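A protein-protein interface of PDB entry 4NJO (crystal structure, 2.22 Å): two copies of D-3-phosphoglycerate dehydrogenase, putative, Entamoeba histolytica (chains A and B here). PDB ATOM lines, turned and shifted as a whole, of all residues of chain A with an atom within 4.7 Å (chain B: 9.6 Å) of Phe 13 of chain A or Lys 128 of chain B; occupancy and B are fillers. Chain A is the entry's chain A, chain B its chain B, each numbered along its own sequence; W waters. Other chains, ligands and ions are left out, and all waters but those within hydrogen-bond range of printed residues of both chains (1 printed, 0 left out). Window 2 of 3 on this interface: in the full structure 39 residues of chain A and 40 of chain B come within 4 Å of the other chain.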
ATOM      1  N   VAL A   7     -34.711   9.128  -6.685  1.00  0.00           N
ATOM      2  CA  VAL A   7     -34.451   7.741  -7.054  1.00  0.00           C
ATOM      3  C   VAL A   7     -35.688   6.889  -6.775  1.00  0.00           C
ATOM      4  O   VAL A   7     -36.014   6.596  -5.621  1.00  0.00           O
ATOM      5  CB  VAL A   7     -33.211   7.174  -6.325  1.00  0.00           C
ATOM      6  CG1 VAL A   7     -32.898   5.766  -6.810  1.00  0.00           C
ATOM      7  CG2 VAL A   7     -32.008   8.085  -6.527  1.00  0.00           C
ATOM      8  N   THR A   9     -37.369   3.542  -6.809  1.00  0.00           N
ATOM      9  CA  THR A   9     -37.130   2.098  -6.807  1.00  0.00           C
ATOM     10  C   THR A   9     -38.065   1.376  -5.839  1.00  0.00           C
ATOM     11  O   THR A   9     -37.813   1.348  -4.630  1.00  0.00           O
ATOM     12  CB  THR A   9     -35.671   1.757  -6.424  1.00  0.00           C
ATOM     13  OG1 THR A   9     -35.358   2.344  -5.155  1.00  0.00           O
ATOM     14  CG2 THR A   9     -34.685   2.262  -7.479  1.00  0.00           C
ATOM     15  N   LYS A  11     -38.471  -1.870  -5.659  1.00  0.00           N
ATOM     16  CA  LYS A  11     -37.503  -2.766  -5.025  1.00  0.00           C
ATOM     17  C   LYS A  11     -36.121  -2.101  -5.015  1.00  0.00           C
ATOM     18  O   LYS A  11     -35.508  -1.915  -6.069  1.00  0.00           O
ATOM     19  CB  LYS A  11     -37.497  -4.185  -5.622  1.00  0.00           C
ATOM     20  CG  LYS A  11     -37.363  -4.306  -7.130  1.00  0.00           C
ATOM     21  CD  LYS A  11     -37.264  -5.777  -7.514  1.00  0.00           C
ATOM     22  CE  LYS A  11     -37.346  -6.001  -9.017  1.00  0.00           C
ATOM     23  NZ  LYS A  11     -36.097  -5.594  -9.721  1.00  0.00           N
ATOM     24  N   PRO A  12     -35.647  -1.719  -3.816  1.00  0.00           N
ATOM     25  CA  PRO A  12     -34.500  -0.822  -3.656  1.00  0.00           C
ATOM     26  C   PRO A  12     -33.174  -1.406  -4.127  1.00  0.00           C
ATOM     27  O   PRO A  12     -33.018  -2.626  -4.186  1.00  0.00           O
ATOM     28  CB  PRO A  12     -34.446  -0.580  -2.139  1.00  0.00           C
ATOM     29  CG  PRO A  12     -35.752  -1.061  -1.603  1.00  0.00           C
ATOM     30  CD  PRO A  12     -36.155  -2.177  -2.513  1.00  0.00           C
ATOM     31  N   PHE A  13     -32.236  -0.522  -4.464  1.00  0.00           N
ATOM     32  CA  PHE A  13     -30.844  -0.896  -4.692  1.00  0.00           C
ATOM     33  C   PHE A  13     -30.234  -1.458  -3.408  1.00  0.00           C
ATOM     34  O   PHE A  13     -30.758  -1.239  -2.309  1.00  0.00           O
ATOM     35  CB  PHE A  13     -30.019   0.326  -5.115  1.00  0.00           C
ATOM     36  CG  PHE A  13     -30.262   0.790  -6.528  1.00  0.00           C
ATOM     37  CD1 PHE A  13     -29.936  -0.017  -7.615  1.00  0.00           C
ATOM     38  CD2 PHE A  13     -30.777   2.057  -6.772  1.00  0.00           C
ATOM     39  CE1 PHE A  13     -30.142   0.422  -8.917  1.00  0.00           C
ATOM     40  CE2 PHE A  13     -30.984   2.504  -8.070  1.00  0.00           C
ATOM     41  CZ  PHE A  13     -30.666   1.685  -9.143  1.00  0.00           C
ATOM     42  N   ALA A  14     -29.125  -2.179  -3.553  1.00  0.00           N
ATOM     43  CA  ALA A  14     -28.288  -2.538  -2.414  1.00  0.00           C
ATOM     44  C   ALA A  14     -27.759  -1.253  -1.776  1.00  0.00           C
ATOM     45  O   ALA A  14     -27.567  -0.246  -2.467  1.00  0.00           O
ATOM     46  CB  ALA A  14     -27.139  -3.431  -2.859  1.00  0.00           C
ATOM     47  N   GLU A  15     -27.536  -1.285  -0.464  1.00  0.00           N
ATOM     48  CA  GLU A  15     -27.088  -0.103   0.281  1.00  0.00           C
ATOM     49  C   GLU A  15     -25.827   0.529  -0.320  1.00  0.00           C
ATOM     50  O   GLU A  15     -25.761   1.748  -0.484  1.00  0.00           O
ATOM     51  CB  GLU A  15     -26.878  -0.439   1.760  1.00  0.00           C
ATOM     52  CG  GLU A  15     -26.683   0.778   2.654  1.00  0.00           C
ATOM     53  CD  GLU A  15     -26.316   0.406   4.079  1.00  0.00           C
ATOM     54  OE1 GLU A  15     -25.212   0.788   4.525  1.00  0.00           O
ATOM     55  OE2 GLU A  15     -27.124  -0.273   4.752  1.00  0.00           O
ATOM     56  N   ALA A  17     -24.847   0.515  -3.350  1.00  0.00           N
ATOM     57  CA  ALA A  17     -25.213   1.207  -4.588  1.00  0.00           C
ATOM     58  C   ALA A  17     -25.818   2.584  -4.300  1.00  0.00           C
ATOM     59  O   ALA A  17     -25.515   3.552  -4.997  1.00  0.00           O
ATOM     60  CB  ALA A  17     -26.168   0.361  -5.419  1.00  0.00           C
ATOM     61  N   VAL A  18     -26.667   2.657  -3.274  1.00  0.00           N
ATOM     62  CA  VAL A  18     -27.226   3.927  -2.791  1.00  0.00           C
ATOM     63  C   VAL A  18     -26.106   4.864  -2.320  1.00  0.00           C
ATOM     64  O   VAL A  18     -26.127   6.063  -2.611  1.00  0.00           O
ATOM     65  CB  VAL A  18     -28.249   3.704  -1.649  1.00  0.00           C
ATOM     66  CG1 VAL A  18     -28.826   5.028  -1.163  1.00  0.00           C
ATOM     67  CG2 VAL A  18     -29.369   2.776  -2.100  1.00  0.00           C
ATOM     68  N   ILE A  21     -24.253   6.176  -5.328  1.00  0.00           N
ATOM     69  CA  ILE A  21     -25.090   7.185  -5.979  1.00  0.00           C
ATOM     70  C   ILE A  21     -24.927   8.539  -5.281  1.00  0.00           C
ATOM     71  O   ILE A  21     -24.759   9.566  -5.943  1.00  0.00           O
ATOM     72  CB  ILE A  21     -26.578   6.748  -6.033  1.00  0.00           C
ATOM     73  CG1 ILE A  21     -26.764   5.616  -7.054  1.00  0.00           C
ATOM     74  CG2 ILE A  21     -27.490   7.920  -6.386  1.00  0.00           C
ATOM     75  CD1 ILE A  21     -28.066   4.849  -6.919  1.00  0.00           C
ATOM     76  N   GLU A  36     -38.320   4.789  -1.951  1.00  0.00           N
ATOM     77  CA  GLU A  36     -38.168   3.336  -1.873  1.00  0.00           C
ATOM     78  C   GLU A  36     -39.395   2.631  -1.306  1.00  0.00           C
ATOM     79  O   GLU A  36     -40.040   3.132  -0.380  1.00  0.00           O
ATOM     80  CB  GLU A  36     -36.938   2.969  -1.041  1.00  0.00           C
ATOM     81  CG  GLU A  36     -35.611   3.370  -1.666  1.00  0.00           C
ATOM     82  CD  GLU A  36     -34.426   3.046  -0.779  1.00  0.00           C
ATOM     83  OE1 GLU A  36     -34.493   3.320   0.438  1.00  0.00           O
ATOM     84  OE2 GLU A  36     -33.419   2.522  -1.297  1.00  0.00           O
ATOM     85  N   ILE A  55     -33.679   8.902 -11.225  1.00  0.00           N
ATOM     86  CA  ILE A  55     -33.100   7.571 -11.413  1.00  0.00           C
ATOM     87  C   ILE A  55     -34.212   6.553 -11.183  1.00  0.00           C
ATOM     88  O   ILE A  55     -34.968   6.665 -10.215  1.00  0.00           O
ATOM     89  CB  ILE A  55     -31.919   7.297 -10.451  1.00  0.00           C
ATOM     90  CG1 ILE A  55     -30.797   8.320 -10.663  1.00  0.00           C
ATOM     91  CG2 ILE A  55     -31.384   5.878 -10.644  1.00  0.00           C
ATOM     92  CD1 ILE A  55     -29.691   8.270  -9.626  1.00  0.00           C
ATOM     93  N   ARG A  57     -35.505   2.137 -11.785  1.00  0.00           N
ATOM     94  CA  ARG A  57     -35.275   0.754 -12.196  1.00  0.00           C
ATOM     95  C   ARG A  57     -36.379   0.276 -13.150  1.00  0.00           C
ATOM     96  O   ARG A  57     -36.630   0.921 -14.166  1.00  0.00           O
ATOM     97  CB  ARG A  57     -35.112  -0.172 -10.985  1.00  0.00           C
ATOM     98  CG  ARG A  57     -33.765  -0.027 -10.297  1.00  0.00           C
ATOM     99  CD  ARG A  57     -33.134  -1.381 -10.029  1.00  0.00           C
ATOM    100  NE  ARG A  57     -33.406  -1.859  -8.682  1.00  0.00           N
ATOM    101  CZ  ARG A  57     -33.147  -3.091  -8.252  1.00  0.00           C
ATOM    102  NH1 ARG A  57     -32.618  -3.997  -9.065  1.00  0.00           N
ATOM    103  NH2 ARG A  57     -33.428  -3.416  -7.002  1.00  0.00           N
ATOM    104  N   ALA A  78     -31.522   2.816 -14.569  1.00  0.00           N
ATOM    105  CA  ALA A  78     -30.361   2.041 -14.161  1.00  0.00           C
ATOM    106  C   ALA A  78     -30.575   0.595 -14.593  1.00  0.00           C
ATOM    107  O   ALA A  78     -31.229  -0.191 -13.899  1.00  0.00           O
ATOM    108  CB  ALA A  78     -30.145   2.145 -12.662  1.00  0.00           C
ATOM    109  N   GLU A 269     -30.740  -8.435  -9.429  1.00  0.00           N
ATOM    110  CA  GLU A 269     -30.762  -8.391  -7.963  1.00  0.00           C
ATOM    111  C   GLU A 269     -29.478  -8.931  -7.332  1.00  0.00           C
ATOM    112  O   GLU A 269     -29.498  -9.915  -6.586  1.00  0.00           O
ATOM    113  CB  GLU A 269     -31.993  -9.121  -7.409  1.00  0.00           C
ATOM    114  CG  GLU A 269     -33.268  -8.295  -7.441  1.00  0.00           C
ATOM    115  CD  GLU A 269     -33.238  -7.149  -6.447  1.00  0.00           C
ATOM    116  OE1 GLU A 269     -33.371  -7.407  -5.231  1.00  0.00           O
ATOM    117  OE2 GLU A 269     -33.077  -5.992  -6.883  1.00  0.00           O
ATOM    118  N   ASN A 274     -26.216  -3.921  -8.985  1.00  0.00           N
ATOM    119  CA  ASN A 274     -26.788  -2.703  -8.399  1.00  0.00           C
ATOM    120  C   ASN A 274     -25.779  -1.557  -8.384  1.00  0.00           C
ATOM    121  O   ASN A 274     -26.099  -0.435  -8.786  1.00  0.00           O
ATOM    122  CB  ASN A 274     -27.297  -2.964  -6.978  1.00  0.00           C
ATOM    123  CG  ASN A 274     -28.659  -3.637  -6.948  1.00  0.00           C
ATOM    124  OD1 ASN A 274     -29.210  -3.875  -5.872  1.00  0.00           O
ATOM    125  ND2 ASN A 274     -29.214  -3.945  -8.121  1.00  0.00           N
ATOM    126  N   GLY A 278     -26.479   1.522 -10.754  1.00  0.00           N
ATOM    127  CA  GLY A 278     -26.785   2.722  -9.977  1.00  0.00           C
ATOM    128  C   GLY A 278     -25.768   3.836 -10.135  1.00  0.00           C
ATOM    129  O   GLY A 278     -26.137   4.992 -10.357  1.00  0.00           O
ATOM    130  N   GLY B 119     -26.975 -21.240  -5.001  1.00  0.00           N
ATOM    131  CA  GLY B 119     -26.686 -20.880  -3.614  1.00  0.00           C
ATOM    132  C   GLY B 119     -26.383 -19.405  -3.441  1.00  0.00           C
ATOM    133  O   GLY B 119     -26.780 -18.793  -2.446  1.00  0.00           O
ATOM    134  N   PHE B 120     -25.674 -18.836  -4.414  1.00  0.00           N
ATOM    135  CA  PHE B 120     -25.337 -17.413  -4.397  1.00  0.00           C
ATOM    136  C   PHE B 120     -26.519 -16.512  -4.748  1.00  0.00           C
ATOM    137  O   PHE B 120     -26.502 -15.320  -4.438  1.00  0.00           O
ATOM    138  CB  PHE B 120     -24.141 -17.125  -5.315  1.00  0.00           C
ATOM    139  CG  PHE B 120     -22.867 -16.798  -4.580  1.00  0.00           C
ATOM    140  CD1 PHE B 120     -22.616 -17.314  -3.310  1.00  0.00           C
ATOM    141  CD2 PHE B 120     -21.906 -15.978  -5.166  1.00  0.00           C
ATOM    142  CE1 PHE B 120     -21.440 -17.015  -2.639  1.00  0.00           C
ATOM    143  CE2 PHE B 120     -20.729 -15.673  -4.500  1.00  0.00           C
ATOM    144  CZ  PHE B 120     -20.496 -16.192  -3.234  1.00  0.00           C
ATOM    145  N   ARG B 121     -27.544 -17.079  -5.382  1.00  0.00           N
ATOM    146  CA  ARG B 121     -28.740 -16.310  -5.735  1.00  0.00           C
ATOM    147  C   ARG B 121     -29.960 -16.722  -4.909  1.00  0.00           C
ATOM    148  O   ARG B 121     -31.090 -16.750  -5.411  1.00  0.00           O
ATOM    149  CB  ARG B 121     -29.025 -16.384  -7.242  1.00  0.00           C
ATOM    150  CG  ARG B 121     -27.872 -15.907  -8.123  1.00  0.00           C
ATOM    151  CD  ARG B 121     -27.597 -14.416  -7.980  1.00  0.00           C
ATOM    152  NE  ARG B 121     -28.482 -13.599  -8.810  1.00  0.00           N
ATOM    153  CZ  ARG B 121     -28.254 -13.297 -10.086  1.00  0.00           C
ATOM    154  NH1 ARG B 121     -27.165 -13.745 -10.703  1.00  0.00           N
ATOM    155  NH2 ARG B 121     -29.116 -12.541 -10.751  1.00  0.00           N
ATOM    156  N   LYS B 122     -29.705 -17.030  -3.635  1.00  0.00           N
ATOM    157  CA  LYS B 122     -30.741 -17.280  -2.610  1.00  0.00           C
ATOM    158  C   LYS B 122     -31.737 -18.389  -2.974  1.00  0.00           C
ATOM    159  O   LYS B 122     -32.904 -18.340  -2.581  1.00  0.00           O
ATOM    160  CB  LYS B 122     -31.499 -15.983  -2.254  1.00  0.00           C
ATOM    161  CG  LYS B 122     -30.653 -14.714  -2.202  1.00  0.00           C
ATOM    162  CD  LYS B 122     -29.906 -14.548  -0.887  1.00  0.00           C
ATOM    163  CE  LYS B 122     -30.716 -13.760   0.128  1.00  0.00           C
ATOM    164  NZ  LYS B 122     -29.917 -13.491   1.355  1.00  0.00           N
ATOM    165  N   GLY B 123     -31.269 -19.389  -3.715  1.00  0.00           N
ATOM    166  CA  GLY B 123     -32.124 -20.483  -4.170  1.00  0.00           C
ATOM    167  C   GLY B 123     -33.156 -20.039  -5.190  1.00  0.00           C
ATOM    168  O   GLY B 123     -34.235 -20.627  -5.290  1.00  0.00           O
ATOM    169  N   LYS B 125     -34.836 -17.281  -5.095  1.00  0.00           N
ATOM    170  CA  LYS B 125     -35.918 -16.560  -4.425  1.00  0.00           C
ATOM    171  C   LYS B 125     -35.532 -15.086  -4.320  1.00  0.00           C
ATOM    172  O   LYS B 125     -34.455 -14.691  -4.773  1.00  0.00           O
ATOM    173  CB  LYS B 125     -36.198 -17.148  -3.031  1.00  0.00           C
ATOM    174  CG  LYS B 125     -36.312 -18.671  -2.958  1.00  0.00           C
ATOM    175  CD  LYS B 125     -37.701 -19.194  -3.310  1.00  0.00           C
ATOM    176  CE  LYS B 125     -37.780 -19.679  -4.751  1.00  0.00           C
ATOM    177  NZ  LYS B 125     -39.003 -20.487  -5.021  1.00  0.00           N
ATOM    178  N   GLU B 126     -36.410 -14.279  -3.725  1.00  0.00           N
ATOM    179  CA  GLU B 126     -36.149 -12.850  -3.533  1.00  0.00           C
ATOM    180  C   GLU B 126     -34.962 -12.614  -2.588  1.00  0.00           C
ATOM    181  O   GLU B 126     -34.594 -13.496  -1.806  1.00  0.00           O
ATOM    182  CB  GLU B 126     -37.406 -12.142  -3.012  1.00  0.00           C
ATOM    183  CG  GLU B 126     -37.399 -10.630  -3.196  1.00  0.00           C
ATOM    184  CD  GLU B 126     -38.743  -9.977  -2.919  1.00  0.00           C
ATOM    185  OE1 GLU B 126     -39.750 -10.698  -2.748  1.00  0.00           O
ATOM    186  OE2 GLU B 126     -38.791  -8.728  -2.881  1.00  0.00           O
ATOM    187  N   GLY B 127     -34.364 -11.428  -2.679  1.00  0.00           N
ATOM    188  CA  GLY B 127     -33.222 -11.058  -1.848  1.00  0.00           C
ATOM    189  C   GLY B 127     -32.014 -10.673  -2.682  1.00  0.00           C
ATOM    190  O   GLY B 127     -31.931 -11.018  -3.863  1.00  0.00           O
ATOM    191  N   LYS B 128     -31.077  -9.955  -2.069  1.00  0.00           N
ATOM    192  CA  LYS B 128     -29.876  -9.522  -2.771  1.00  0.00           C
ATOM    193  C   LYS B 128     -28.874 -10.663  -2.886  1.00  0.00           C
ATOM    194  O   LYS B 128     -28.287 -11.092  -1.894  1.00  0.00           O
ATOM    195  CB  LYS B 128     -29.243  -8.301  -2.092  1.00  0.00           C
ATOM    196  CG  LYS B 128     -30.089  -7.035  -2.142  1.00  0.00           C
ATOM    197  CD  LYS B 128     -30.242  -6.492  -3.558  1.00  0.00           C
ATOM    198  CE  LYS B 128     -31.095  -5.232  -3.580  1.00  0.00           C
ATOM    199  NZ  LYS B 128     -32.471  -5.445  -3.046  1.00  0.00           N
ATOM    200  N   GLY B 129     -28.694 -11.156  -4.108  1.00  0.00           N
ATOM    201  CA  GLY B 129     -27.758 -12.243  -4.369  1.00  0.00           C
ATOM    202  C   GLY B 129     -26.351 -11.743  -4.627  1.00  0.00           C
ATOM    203  O   GLY B 129     -26.081 -10.544  -4.550  1.00  0.00           O
ATOM    204  N   ARG B 130     -25.448 -12.671  -4.922  1.00  0.00           N
ATOM    205  CA  ARG B 130     -24.087 -12.314  -5.309  1.00  0.00           C
ATOM    206  C   ARG B 130     -23.685 -12.997  -6.609  1.00  0.00           C
ATOM    207  O   ARG B 130     -24.313 -13.966  -7.034  1.00  0.00           O
ATOM    208  CB  ARG B 130     -23.090 -12.637  -4.191  1.00  0.00           C
ATOM    209  CG  ARG B 130     -23.062 -11.601  -3.077  1.00  0.00           C
ATOM    210  CD  ARG B 130     -21.672 -11.477  -2.473  1.00  0.00           C
ATOM    211  NE  ARG B 130     -21.369 -12.576  -1.562  1.00  0.00           N
ATOM    212  CZ  ARG B 130     -20.169 -12.821  -1.039  1.00  0.00           C
ATOM    213  NH1 ARG B 130     -19.129 -12.046  -1.327  1.00  0.00           N
ATOM    214  NH2 ARG B 130     -20.010 -13.852  -0.221  1.00  0.00           N
ATOM    215  N   GLU B 131     -22.635 -12.478  -7.237  1.00  0.00           N
ATOM    216  CA  GLU B 131     -22.120 -13.044  -8.478  1.00  0.00           C
ATOM    217  C   GLU B 131     -20.846 -13.842  -8.223  1.00  0.00           C
ATOM    218  O   GLU B 131     -20.047 -13.488  -7.356  1.00  0.00           O
ATOM    219  CB  GLU B 131     -21.873 -11.937  -9.506  1.00  0.00           C
ATOM    220  CG  GLU B 131     -23.145 -11.260  -9.994  1.00  0.00           C
ATOM    221  CD  GLU B 131     -22.895  -9.953 -10.728  1.00  0.00           C
ATOM    222  OE1 GLU B 131     -21.787  -9.763 -11.276  1.00  0.00           O
ATOM    223  OE2 GLU B 131     -23.818  -9.112 -10.766  1.00  0.00           O
ATOM    224  N   TYR B 210     -16.800 -13.342   4.372  1.00  0.00           N
ATOM    225  CA  TYR B 210     -18.228 -13.029   4.423  1.00  0.00           C
ATOM    226  C   TYR B 210     -19.005 -13.725   3.305  1.00  0.00           C
ATOM    227  O   TYR B 210     -18.595 -13.707   2.142  1.00  0.00           O
ATOM    228  CB  TYR B 210     -18.501 -11.518   4.384  1.00  0.00           C
ATOM    229  CG  TYR B 210     -19.989 -11.222   4.340  1.00  0.00           C
ATOM    230  CD1 TYR B 210     -20.762 -11.285   5.500  1.00  0.00           C
ATOM    231  CD2 TYR B 210     -20.632 -10.931   3.134  1.00  0.00           C
ATOM    232  CE1 TYR B 210     -22.125 -11.043   5.466  1.00  0.00           C
ATOM    233  CE2 TYR B 210     -21.999 -10.691   3.090  1.00  0.00           C
ATOM    234  CZ  TYR B 210     -22.737 -10.747   4.261  1.00  0.00           C
ATOM    235  OH  TYR B 210     -24.091 -10.507   4.239  1.00  0.00           O
ATOM    236  N   GLY B 211     -20.130 -14.331   3.681  1.00  0.00           N
ATOM    237  CA  GLY B 211     -21.001 -15.030   2.739  1.00  0.00           C
ATOM    238  C   GLY B 211     -20.355 -16.254   2.117  1.00  0.00           C
ATOM    239  O   GLY B 211     -20.669 -16.618   0.981  1.00  0.00           O
ATOM    240  N   ILE B 239     -23.236 -20.283   3.665  1.00  0.00           N
ATOM    241  CA  ILE B 239     -24.117 -21.057   2.801  1.00  0.00           C
ATOM    242  C   ILE B 239     -23.528 -22.448   2.572  1.00  0.00           C
ATOM    243  O   ILE B 239     -22.337 -22.590   2.277  1.00  0.00           O
ATOM    244  CB  ILE B 239     -24.344 -20.353   1.441  1.00  0.00           C
ATOM    245  CG1 ILE B 239     -24.768 -18.893   1.645  1.00  0.00           C
ATOM    246  CG2 ILE B 239     -25.380 -21.102   0.608  1.00  0.00           C
ATOM    247  CD1 ILE B 239     -24.586 -18.007   0.428  1.00  0.00           C
ATOM    248  N   GLY B 257     -32.906 -20.607   3.357  1.00  0.00           N
ATOM    249  CA  GLY B 257     -32.404 -19.432   2.651  1.00  0.00           C
ATOM    250  C   GLY B 257     -30.900 -19.476   2.431  1.00  0.00           C
ATOM    251  O   GLY B 257     -30.354 -18.647   1.701  1.00  0.00           O
HETATM  252  O   HOH W   1     -30.281 -12.611  -7.067  1.00  0.00           O
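NZ of Lys 128 of chain B is in hydrogen-bond range of O of Pro 12 of chain A, 3.1 Å away. The side-chain amino group (NZ) of Lys 128 of chain B lies within salt-bridge range of the side-chain carboxylate (OE1) of Glu 269 of chain A. N of Gly 129 of chain B sits at hydrogen-bond distance from O of Glu 269 of chain A (2.9 Å).
Of the 16 printed residues of chain B, 3 touch a printed residue of chain A. Printed residues of chain A that touch a printed residue of chain B: Pro 12, Phe 13, Ala 14, Glu 269 and Asn 274. Along chain A the printed residues that touch a printed residue of chain B span positions 12 to 274. Among the printed residues, 7 pairs touch across the chains.
No position is printed for both chains. Of the 7 pairs that touch across the chains among the printed residues, none has its exchanged pair printed and touching as well.
Phe 13 of chain A touches just one residue of chain B: Lys 128 (3.9 Å). Lys 128 of chain B touches just these residues of chain A: Pro 12, Phe 13, Ala 14, Glu 269 and Asn 274. Of chain B, only Lys 128 (3.1 Å) comes within 4 Å of Pro 12 of chain A. No residue of chain B comes within 4 Å of Ala 17 of chain A. Of the printed residues of chain B, Asn 274 of chain A touches Lys 128 (3.3 Å). Printed residues of chain A within 4 Å of Gly 127 of chain B: Glu 269 (3.8 Å). Of the printed residues of chain A, Gly 129 of chain B touches Glu 269 (2.9 Å). Gly 119 of chain B touches none of the printed residues of chain A. Arg 57 of chain A touches none of the printed residues of chain B. The nearest residue of chain B that does not touch Phe 13 of chain A is Gly 127 of chain B (9.4 Å). The nearest residue of chain A that does not touch Lys 128 of chain B is Arg 57 of chain A (4.5 Å).
The backbone carbonyl oxygen (O) of Pro 12 of chain A is in hydrogen-bond range of the guanidinium group (NH2) of Arg 57 of chain A, 3.0 Å away. The backbone NH (N) of Ala 14 of chain A is in hydrogen-bond range of the side-chain amide oxygen (OD1) of Asn 274 of chain A. OE2 of Glu 269 of chain A lies within salt-bridge range of NH2 of Arg 57 of chain A, at 2.6 Å.
Among the printed residues, merely in contact across the chains: Asn 274 of chain A with Lys 128 of chain B (3.3 Å), Ala 14 of chain A with Lys 128 of chain B (3.6 Å), Glu 269 of chain A with Gly 127 of chain B (3.8 Å) and Phe 13 of chain A with Lys 128 of chain B (3.9 Å).
Water W1 bridges the guanidinium group (NE) of Arg 121 of chain B and the backbone carbonyl oxygen (O) of Glu 269 of chain A.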
